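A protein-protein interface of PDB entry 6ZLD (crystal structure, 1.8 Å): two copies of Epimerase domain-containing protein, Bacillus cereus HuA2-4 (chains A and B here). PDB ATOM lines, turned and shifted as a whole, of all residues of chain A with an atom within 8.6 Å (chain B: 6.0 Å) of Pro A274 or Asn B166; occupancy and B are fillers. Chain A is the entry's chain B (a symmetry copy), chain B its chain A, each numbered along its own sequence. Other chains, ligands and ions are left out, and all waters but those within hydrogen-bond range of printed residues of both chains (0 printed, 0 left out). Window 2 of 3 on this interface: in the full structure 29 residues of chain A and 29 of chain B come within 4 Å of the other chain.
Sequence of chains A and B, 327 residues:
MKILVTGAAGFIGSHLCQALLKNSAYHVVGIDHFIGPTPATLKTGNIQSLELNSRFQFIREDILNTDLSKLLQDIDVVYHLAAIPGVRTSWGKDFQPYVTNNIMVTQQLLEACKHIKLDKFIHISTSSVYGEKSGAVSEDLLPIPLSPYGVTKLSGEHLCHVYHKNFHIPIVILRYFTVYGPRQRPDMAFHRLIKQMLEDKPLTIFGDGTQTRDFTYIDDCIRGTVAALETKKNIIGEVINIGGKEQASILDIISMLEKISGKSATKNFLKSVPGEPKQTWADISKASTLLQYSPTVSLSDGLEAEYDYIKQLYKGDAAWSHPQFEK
ND2 of Asn B166 sits close to N of Gly A275, at 3.0 Å. O of Leu A146 lies close to OD1 of Asn B166 (2.8 Å).
The backbone carbonyl oxygen (O) of Val B162 lies close to the side-chain amide oxygen (OD1) of Asn B166 (2.9 Å). The backbone carbonyl oxygen (O) of Tyr B163 is in hydrogen-bond range of the backbone NH (N) of His B168, 3.3 Å away.
Trp A91 touches Val B162 (CH2 to CG1, 3.5 Å). Trp A91 touches Tyr B163. Asn B166 touches Trp A91 (OD1 to CH2, 3.8 Å). Trp A91 touches Phe B167 (CZ3 to CE2, 3.4 Å). Ile A144 touches His B161. O of Pro A145 touches CG2 of Val B162, 3.3 Å away. O of Leu A146 touches CG1 of Val B162, 3.6 Å away. Lys B165 touches Leu A146 (CE to CD2, 3.5 Å). Pro A148 touches Val B162. ND2 of Asn B166 touches CA of Pro A274, at 3.7 Å.
Printed residues of chain B within 4 Å of Pro A148: Val B162. Of the printed residues of chain B, Gly A275 touches Asn B166 (3.0 Å). Pro A277 touches none of the printed residues of chain B. His B164 touches none of the printed residues of chain A. Asn B166 touches just these residues of chain A: Trp A91, Leu A146, Pro A274 and Gly A275. Printed residues of chain A within 4 Å of Phe B167: Trp A91.
Of the 18 printed residues of chain A, 8 touch a printed residue of chain B. Printed residues of chain A that touch a printed residue of chain B: Trp A91, Ile A144, Pro A145, Leu A146, Ser A147, Pro A148, Pro A274 and Gly A275. Hydrophobic or aromatic side chains of chain B that line the printed part of chain A: His B161, Val B162, Tyr B163 and Phe B167. Along chain B the printed residues that touch a printed residue of chain A span positions 161 to 167.
No position is printed for both chains.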
ATOM      1  N   VAL A  87      17.390  18.049  10.462  1.00  0.00           N
ATOM      2  CA  VAL A  87      17.323  17.255  11.722  1.00  0.00           C
ATOM      3  C   VAL A  87      18.392  17.753  12.703  1.00  0.00           C
ATOM      4  O   VAL A  87      18.116  17.820  13.904  1.00  0.00           O
ATOM      5  CB  VAL A  87      17.479  15.750  11.452  1.00  0.00           C
ATOM      6  CG1 VAL A  87      17.503  14.961  12.749  1.00  0.00           C
ATOM      7  CG2 VAL A  87      16.397  15.243  10.533  1.00  0.00           C
ATOM      8  N   ARG A  88      19.570  18.078  12.181  1.00  0.00           N
ATOM      9  CA  ARG A  88      20.829  18.182  12.951  1.00  0.00           C
ATOM     10  C   ARG A  88      21.045  19.587  13.498  1.00  0.00           C
ATOM     11  O   ARG A  88      21.943  19.727  14.362  1.00  0.00           O
ATOM     12  CB  ARG A  88      22.003  17.750  12.059  1.00  0.00           C
ATOM     13  CG  ARG A  88      22.004  16.245  11.809  1.00  0.00           C
ATOM     14  CD  ARG A  88      23.156  15.770  10.941  1.00  0.00           C
ATOM     15  NE  ARG A  88      22.976  16.201   9.561  1.00  0.00           N
ATOM     16  CZ  ARG A  88      22.185  15.611   8.669  1.00  0.00           C
ATOM     17  NH1 ARG A  88      22.121  16.106   7.449  1.00  0.00           N
ATOM     18  NH2 ARG A  88      21.476  14.538   8.990  1.00  0.00           N
ATOM     19  N   THR A  89      20.288  20.589  13.049  1.00  0.00           N
ATOM     20  CA  THR A  89      20.586  22.008  13.358  1.00  0.00           C
ATOM     21  C   THR A  89      19.440  22.623  14.170  1.00  0.00           C
ATOM     22  O   THR A  89      19.182  23.836  13.978  1.00  0.00           O
ATOM     23  CB  THR A  89      20.841  22.803  12.067  1.00  0.00           C
ATOM     24  OG1 THR A  89      19.708  22.645  11.198  1.00  0.00           O
ATOM     25  CG2 THR A  89      22.097  22.365  11.342  1.00  0.00           C
ATOM     26  N   SER A  90      18.764  21.830  15.014  1.00  0.00           N
ATOM     27  CA  SER A  90      17.537  22.287  15.725  1.00  0.00           C
ATOM     28  C   SER A  90      17.781  22.485  17.228  1.00  0.00           C
ATOM     29  O   SER A  90      16.778  22.568  17.956  1.00  0.00           O
ATOM     30  CB  SER A  90      16.358  21.372  15.467  1.00  0.00           C
ATOM     31  OG  SER A  90      16.525  20.045  15.952  1.00  0.00           O
ATOM     32  N   TRP A  91      19.039  22.562  17.677  1.00  0.00           N
ATOM     33  CA  TRP A  91      19.428  22.666  19.118  1.00  0.00           C
ATOM     34  C   TRP A  91      19.631  24.114  19.547  1.00  0.00           C
ATOM     35  O   TRP A  91      19.957  24.988  18.706  1.00  0.00           O
ATOM     36  CB  TRP A  91      20.697  21.852  19.430  1.00  0.00           C
ATOM     37  CG  TRP A  91      20.577  20.407  19.078  1.00  0.00           C
ATOM     38  CD1 TRP A  91      21.098  19.793  17.978  1.00  0.00           C
ATOM     39  CD2 TRP A  91      19.852  19.397  19.796  1.00  0.00           C
ATOM     40  NE1 TRP A  91      20.773  18.462  17.975  1.00  0.00           N
ATOM     41  CE2 TRP A  91      19.999  18.194  19.074  1.00  0.00           C
ATOM     42  CE3 TRP A  91      19.138  19.373  21.001  1.00  0.00           C
ATOM     43  CZ2 TRP A  91      19.456  16.996  19.524  1.00  0.00           C
ATOM     44  CZ3 TRP A  91      18.595  18.189  21.429  1.00  0.00           C
ATOM     45  CH2 TRP A  91      18.742  17.017  20.693  1.00  0.00           C
ATOM     46  N   ILE A 144       7.868   8.964  19.221  1.00  0.00           N
ATOM     47  CA  ILE A 144       8.756   9.587  20.227  1.00  0.00           C
ATOM     48  C   ILE A 144       9.950  10.151  19.468  1.00  0.00           C
ATOM     49  O   ILE A 144      10.945   9.461  19.184  1.00  0.00           O
ATOM     50  CB  ILE A 144       9.119   8.634  21.381  1.00  0.00           C
ATOM     51  CG1 ILE A 144       7.877   8.027  22.044  1.00  0.00           C
ATOM     52  CG2 ILE A 144       9.924   9.380  22.421  1.00  0.00           C
ATOM     53  CD1 ILE A 144       7.140   9.004  22.947  1.00  0.00           C
ATOM     54  N   PRO A 145       9.821  11.423  19.029  1.00  0.00           N
ATOM     55  CA  PRO A 145      10.882  12.080  18.270  1.00  0.00           C
ATOM     56  C   PRO A 145      12.197  12.095  19.053  1.00  0.00           C
ATOM     57  O   PRO A 145      12.168  12.247  20.261  1.00  0.00           O
ATOM     58  CB  PRO A 145      10.387  13.517  18.037  1.00  0.00           C
ATOM     59  CG  PRO A 145       8.912  13.498  18.365  1.00  0.00           C
ATOM     60  CD  PRO A 145       8.636  12.277  19.224  1.00  0.00           C
ATOM     61  N   LEU A 146      13.313  11.988  18.333  1.00  0.00           N
ATOM     62  CA  LEU A 146      14.691  12.046  18.876  1.00  0.00           C
ATOM     63  C   LEU A 146      15.267  13.450  18.783  1.00  0.00           C
ATOM     64  O   LEU A 146      16.302  13.682  19.430  1.00  0.00           O
ATOM     65  CB  LEU A 146      15.597  11.158  18.022  1.00  0.00           C
ATOM     66  CG  LEU A 146      15.642   9.664  18.311  1.00  0.00           C
ATOM     67  CD1 LEU A 146      17.078   9.186  18.113  1.00  0.00           C
ATOM     68  CD2 LEU A 146      15.155   9.320  19.706  1.00  0.00           C
ATOM     69  N   SER A 147      14.724  14.317  17.922  1.00  0.00           N
ATOM     70  CA  SER A 147      15.261  15.679  17.658  1.00  0.00           C
ATOM     71  C   SER A 147      14.224  16.757  17.957  1.00  0.00           C
ATOM     72  O   SER A 147      13.034  16.521  17.816  1.00  0.00           O
ATOM     73  CB  SER A 147      15.709  15.847  16.233  1.00  0.00           C
ATOM     74  OG  SER A 147      14.634  15.656  15.307  1.00  0.00           O
ATOM     75  N   PRO A 148      14.656  17.964  18.350  1.00  0.00           N
ATOM     76  CA  PRO A 148      13.746  19.109  18.493  1.00  0.00           C
ATOM     77  C   PRO A 148      12.953  19.343  17.205  1.00  0.00           C
ATOM     78  O   PRO A 148      11.791  19.654  17.286  1.00  0.00           O
ATOM     79  CB  PRO A 148      14.703  20.256  18.819  1.00  0.00           C
ATOM     80  CG  PRO A 148      15.801  19.556  19.570  1.00  0.00           C
ATOM     81  CD  PRO A 148      16.020  18.287  18.783  1.00  0.00           C
ATOM     82  N   PHE A 206      28.767  10.795   9.622  1.00  0.00           N
ATOM     83  CA  PHE A 206      28.418  11.146  11.027  1.00  0.00           C
ATOM     84  C   PHE A 206      28.116   9.862  11.816  1.00  0.00           C
ATOM     85  O   PHE A 206      26.912   9.530  11.978  1.00  0.00           O
ATOM     86  CB  PHE A 206      27.234  12.122  11.092  1.00  0.00           C
ATOM     87  CG  PHE A 206      27.419  13.414  10.335  1.00  0.00           C
ATOM     88  CD1 PHE A 206      28.688  13.894  10.015  1.00  0.00           C
ATOM     89  CD2 PHE A 206      26.321  14.141   9.915  1.00  0.00           C
ATOM     90  CE1 PHE A 206      28.846  15.076   9.304  1.00  0.00           C
ATOM     91  CE2 PHE A 206      26.476  15.320   9.210  1.00  0.00           C
ATOM     92  CZ  PHE A 206      27.731  15.795   8.912  1.00  0.00           C
ATOM     93  N   LYS A 271      32.210  12.148  14.531  1.00  0.00           N
ATOM     94  CA  LYS A 271      31.373  11.819  15.705  1.00  0.00           C
ATOM     95  C   LYS A 271      29.920  11.778  15.240  1.00  0.00           C
ATOM     96  O   LYS A 271      29.509  12.691  14.544  1.00  0.00           O
ATOM     97  CB  LYS A 271      31.553  12.851  16.823  1.00  0.00           C
ATOM     98  CG  LYS A 271      32.397  12.380  17.993  1.00  0.00           C
ATOM     99  CD  LYS A 271      31.566  11.897  19.182  1.00  0.00           C
ATOM    100  CE  LYS A 271      32.231  12.133  20.526  1.00  0.00           C
ATOM    101  NZ  LYS A 271      33.362  11.205  20.781  1.00  0.00           N
ATOM    102  N   SER A 272      29.186  10.750  15.637  1.00  0.00           N
ATOM    103  CA  SER A 272      27.714  10.737  15.532  1.00  0.00           C
ATOM    104  C   SER A 272      27.197  12.012  16.210  1.00  0.00           C
ATOM    105  O   SER A 272      27.863  12.508  17.165  1.00  0.00           O
ATOM    106  CB  SER A 272      27.129   9.472  16.112  1.00  0.00           C
ATOM    107  OG  SER A 272      27.225   9.452  17.529  1.00  0.00           O
ATOM    108  N   VAL A 273      26.088  12.531  15.688  1.00  0.00           N
ATOM    109  CA  VAL A 273      25.451  13.844  16.015  1.00  0.00           C
ATOM    110  C   VAL A 273      24.158  13.535  16.761  1.00  0.00           C
ATOM    111  O   VAL A 273      23.412  12.651  16.347  1.00  0.00           O
ATOM    112  CB  VAL A 273      25.182  14.629  14.714  1.00  0.00           C
ATOM    113  CG1 VAL A 273      23.936  15.498  14.777  1.00  0.00           C
ATOM    114  CG2 VAL A 273      26.396  15.464  14.309  1.00  0.00           C
ATOM    115  N   PRO A 274      23.840  14.248  17.864  1.00  0.00           N
ATOM    116  CA  PRO A 274      22.608  13.971  18.599  1.00  0.00           C
ATOM    117  C   PRO A 274      21.351  14.163  17.744  1.00  0.00           C
ATOM    118  O   PRO A 274      21.348  15.004  16.843  1.00  0.00           O
ATOM    119  CB  PRO A 274      22.609  14.971  19.771  1.00  0.00           C
ATOM    120  CG  PRO A 274      23.693  15.979  19.467  1.00  0.00           C
ATOM    121  CD  PRO A 274      24.644  15.310  18.486  1.00  0.00           C
ATOM    122  N   GLY A 275      20.309  13.424  18.084  1.00  0.00           N
ATOM    123  CA  GLY A 275      18.944  13.667  17.583  1.00  0.00           C
ATOM    124  C   GLY A 275      18.646  12.884  16.322  1.00  0.00           C
ATOM    125  O   GLY A 275      17.547  13.053  15.797  1.00  0.00           O
ATOM    126  N   GLU A 276      19.546  11.999  15.889  1.00  0.00           N
ATOM    127  CA  GLU A 276      19.394  11.207  14.638  1.00  0.00           C
ATOM    128  C   GLU A 276      19.097   9.752  14.976  1.00  0.00           C
ATOM    129  O   GLU A 276      19.884   9.126  15.679  1.00  0.00           O
ATOM    130  CB  GLU A 276      20.698  11.216  13.837  1.00  0.00           C
ATOM    131  CG  GLU A 276      21.185  12.590  13.476  1.00  0.00           C
ATOM    132  CD  GLU A 276      21.830  12.589  12.113  1.00  0.00           C
ATOM    133  OE1 GLU A 276      23.051  12.273  12.024  1.00  0.00           O
ATOM    134  OE2 GLU A 276      21.087  12.840  11.159  1.00  0.00           O
ATOM    135  N   PRO A 277      18.036   9.123  14.416  1.00  0.00           N
ATOM    136  CA  PRO A 277      17.881   7.671  14.545  1.00  0.00           C
ATOM    137  C   PRO A 277      18.917   6.894  13.717  1.00  0.00           C
ATOM    138  O   PRO A 277      19.387   7.403  12.737  1.00  0.00           O
ATOM    139  CB  PRO A 277      16.482   7.421  13.964  1.00  0.00           C
ATOM    140  CG  PRO A 277      16.367   8.499  12.899  1.00  0.00           C
ATOM    141  CD  PRO A 277      16.996   9.720  13.552  1.00  0.00           C
ATOM    142  N   HIS B 161      11.789  13.925  26.541  1.00  0.00           N
ATOM    143  CA  HIS B 161      12.303  12.655  25.967  1.00  0.00           C
ATOM    144  C   HIS B 161      13.528  12.929  25.087  1.00  0.00           C
ATOM    145  O   HIS B 161      14.520  12.168  25.213  1.00  0.00           O
ATOM    146  CB  HIS B 161      11.223  11.877  25.207  1.00  0.00           C
ATOM    147  CG  HIS B 161      10.094  11.425  26.064  1.00  0.00           C
ATOM    148  ND1 HIS B 161      10.298  10.705  27.224  1.00  0.00           N
ATOM    149  CD2 HIS B 161       8.761  11.618  25.975  1.00  0.00           C
ATOM    150  CE1 HIS B 161       9.135  10.438  27.794  1.00  0.00           C
ATOM    151  NE2 HIS B 161       8.184  10.995  27.059  1.00  0.00           N
ATOM    152  N   VAL B 162      13.486  13.968  24.254  1.00  0.00           N
ATOM    153  CA  VAL B 162      14.637  14.300  23.375  1.00  0.00           C
ATOM    154  C   VAL B 162      15.861  14.555  24.268  1.00  0.00           C
ATOM    155  O   VAL B 162      16.957  14.035  23.976  1.00  0.00           O
ATOM    156  CB  VAL B 162      14.319  15.517  22.482  1.00  0.00           C
ATOM    157  CG1 VAL B 162      15.556  16.159  21.921  1.00  0.00           C
ATOM    158  CG2 VAL B 162      13.329  15.173  21.369  1.00  0.00           C
ATOM    159  N   TYR B 163      15.719  15.359  25.312  1.00  0.00           N
ATOM    160  CA  TYR B 163      16.890  15.791  26.118  1.00  0.00           C
ATOM    161  C   TYR B 163      17.357  14.668  27.058  1.00  0.00           C
ATOM    162  O   TYR B 163      18.603  14.607  27.315  1.00  0.00           O
ATOM    163  CB  TYR B 163      16.615  17.133  26.770  1.00  0.00           C
ATOM    164  CG  TYR B 163      16.804  18.298  25.827  1.00  0.00           C
ATOM    165  CD1 TYR B 163      15.789  18.649  24.950  1.00  0.00           C
ATOM    166  CD2 TYR B 163      17.938  19.094  25.847  1.00  0.00           C
ATOM    167  CE1 TYR B 163      15.930  19.699  24.065  1.00  0.00           C
ATOM    168  CE2 TYR B 163      18.093  20.164  24.969  1.00  0.00           C
ATOM    169  CZ  TYR B 163      17.095  20.443  24.051  1.00  0.00           C
ATOM    170  OH  TYR B 163      17.158  21.504  23.195  1.00  0.00           O
ATOM    171  N   HIS B 164      16.437  13.826  27.557  1.00  0.00           N
ATOM    172  CA  HIS B 164      16.785  12.609  28.335  1.00  0.00           C
ATOM    173  C   HIS B 164      17.642  11.696  27.452  1.00  0.00           C
ATOM    174  O   HIS B 164      18.767  11.377  27.862  1.00  0.00           O
ATOM    175  CB  HIS B 164      15.523  11.903  28.850  1.00  0.00           C
ATOM    176  CG  HIS B 164      15.787  10.579  29.487  1.00  0.00           C
ATOM    177  ND1 HIS B 164      15.066   9.439  29.153  1.00  0.00           N
ATOM    178  CD2 HIS B 164      16.733  10.187  30.375  1.00  0.00           C
ATOM    179  CE1 HIS B 164      15.554   8.410  29.832  1.00  0.00           C
ATOM    180  NE2 HIS B 164      16.566   8.841  30.595  1.00  0.00           N
ATOM    181  N   LYS B 165      17.133  11.315  26.275  1.00  0.00           N
ATOM    182  CA  LYS B 165      17.756  10.288  25.398  1.00  0.00           C
ATOM    183  C   LYS B 165      19.118  10.745  24.861  1.00  0.00           C
ATOM    184  O   LYS B 165      19.973   9.862  24.682  1.00  0.00           O
ATOM    185  CB  LYS B 165      16.813   9.859  24.279  1.00  0.00           C
ATOM    186  CG  LYS B 165      15.852   8.766  24.706  1.00  0.00           C
ATOM    187  CD  LYS B 165      15.351   7.873  23.585  1.00  0.00           C
ATOM    188  CE  LYS B 165      14.110   8.422  22.908  1.00  0.00           C
ATOM    189  NZ  LYS B 165      13.006   8.660  23.878  1.00  0.00           N
ATOM    190  N   ASN B 166      19.300  12.034  24.576  1.00  0.00           N
ATOM    191  CA  ASN B 166      20.500  12.589  23.904  1.00  0.00           C
ATOM    192  C   ASN B 166      21.534  13.032  24.938  1.00  0.00           C
ATOM    193  O   ASN B 166      22.716  12.834  24.669  1.00  0.00           O
ATOM    194  CB  ASN B 166      20.140  13.711  22.936  1.00  0.00           C
ATOM    195  CG  ASN B 166      19.435  13.166  21.705  1.00  0.00           C
ATOM    196  OD1 ASN B 166      18.228  13.362  21.490  1.00  0.00           O
ATOM    197  ND2 ASN B 166      20.173  12.437  20.905  1.00  0.00           N
ATOM    198  N   PHE B 167      21.109  13.606  26.056  1.00  0.00           N
ATOM    199  CA  PHE B 167      22.001  14.311  27.010  1.00  0.00           C
ATOM    200  C   PHE B 167      21.831  13.749  28.421  1.00  0.00           C
ATOM    201  O   PHE B 167      22.458  14.325  29.328  1.00  0.00           O
ATOM    202  CB  PHE B 167      21.767  15.826  26.974  1.00  0.00           C
ATOM    203  CG  PHE B 167      21.983  16.433  25.614  1.00  0.00           C
ATOM    204  CD1 PHE B 167      23.248  16.471  25.061  1.00  0.00           C
ATOM    205  CD2 PHE B 167      20.928  16.945  24.871  1.00  0.00           C
ATOM    206  CE1 PHE B 167      23.460  17.001  23.798  1.00  0.00           C
ATOM    207  CE2 PHE B 167      21.142  17.469  23.603  1.00  0.00           C
ATOM    208  CZ  PHE B 167      22.407  17.492  23.062  1.00  0.00           C
ATOM    209  N   HIS B 168      21.012  12.712  28.589  1.00  0.00           N
ATOM    210  CA  HIS B 168      20.825  12.000  29.881  1.00  0.00           C
ATOM    211  C   HIS B 168      20.309  12.978  30.941  1.00  0.00           C
ATOM    212  O   HIS B 168      20.619  12.799  32.124  1.00  0.00           O
ATOM    213  CB  HIS B 168      22.141  11.316  30.295  1.00  0.00           C
ATOM    214  CG  HIS B 168      22.691  10.450  29.213  1.00  0.00           C
ATOM    215  ND1 HIS B 168      21.954   9.412  28.656  1.00  0.00           N
ATOM    216  CD2 HIS B 168      23.870  10.490  28.546  1.00  0.00           C
ATOM    217  CE1 HIS B 168      22.663   8.831  27.706  1.00  0.00           C
ATOM    218  NE2 HIS B 168      23.844   9.477  27.617  1.00  0.00           N
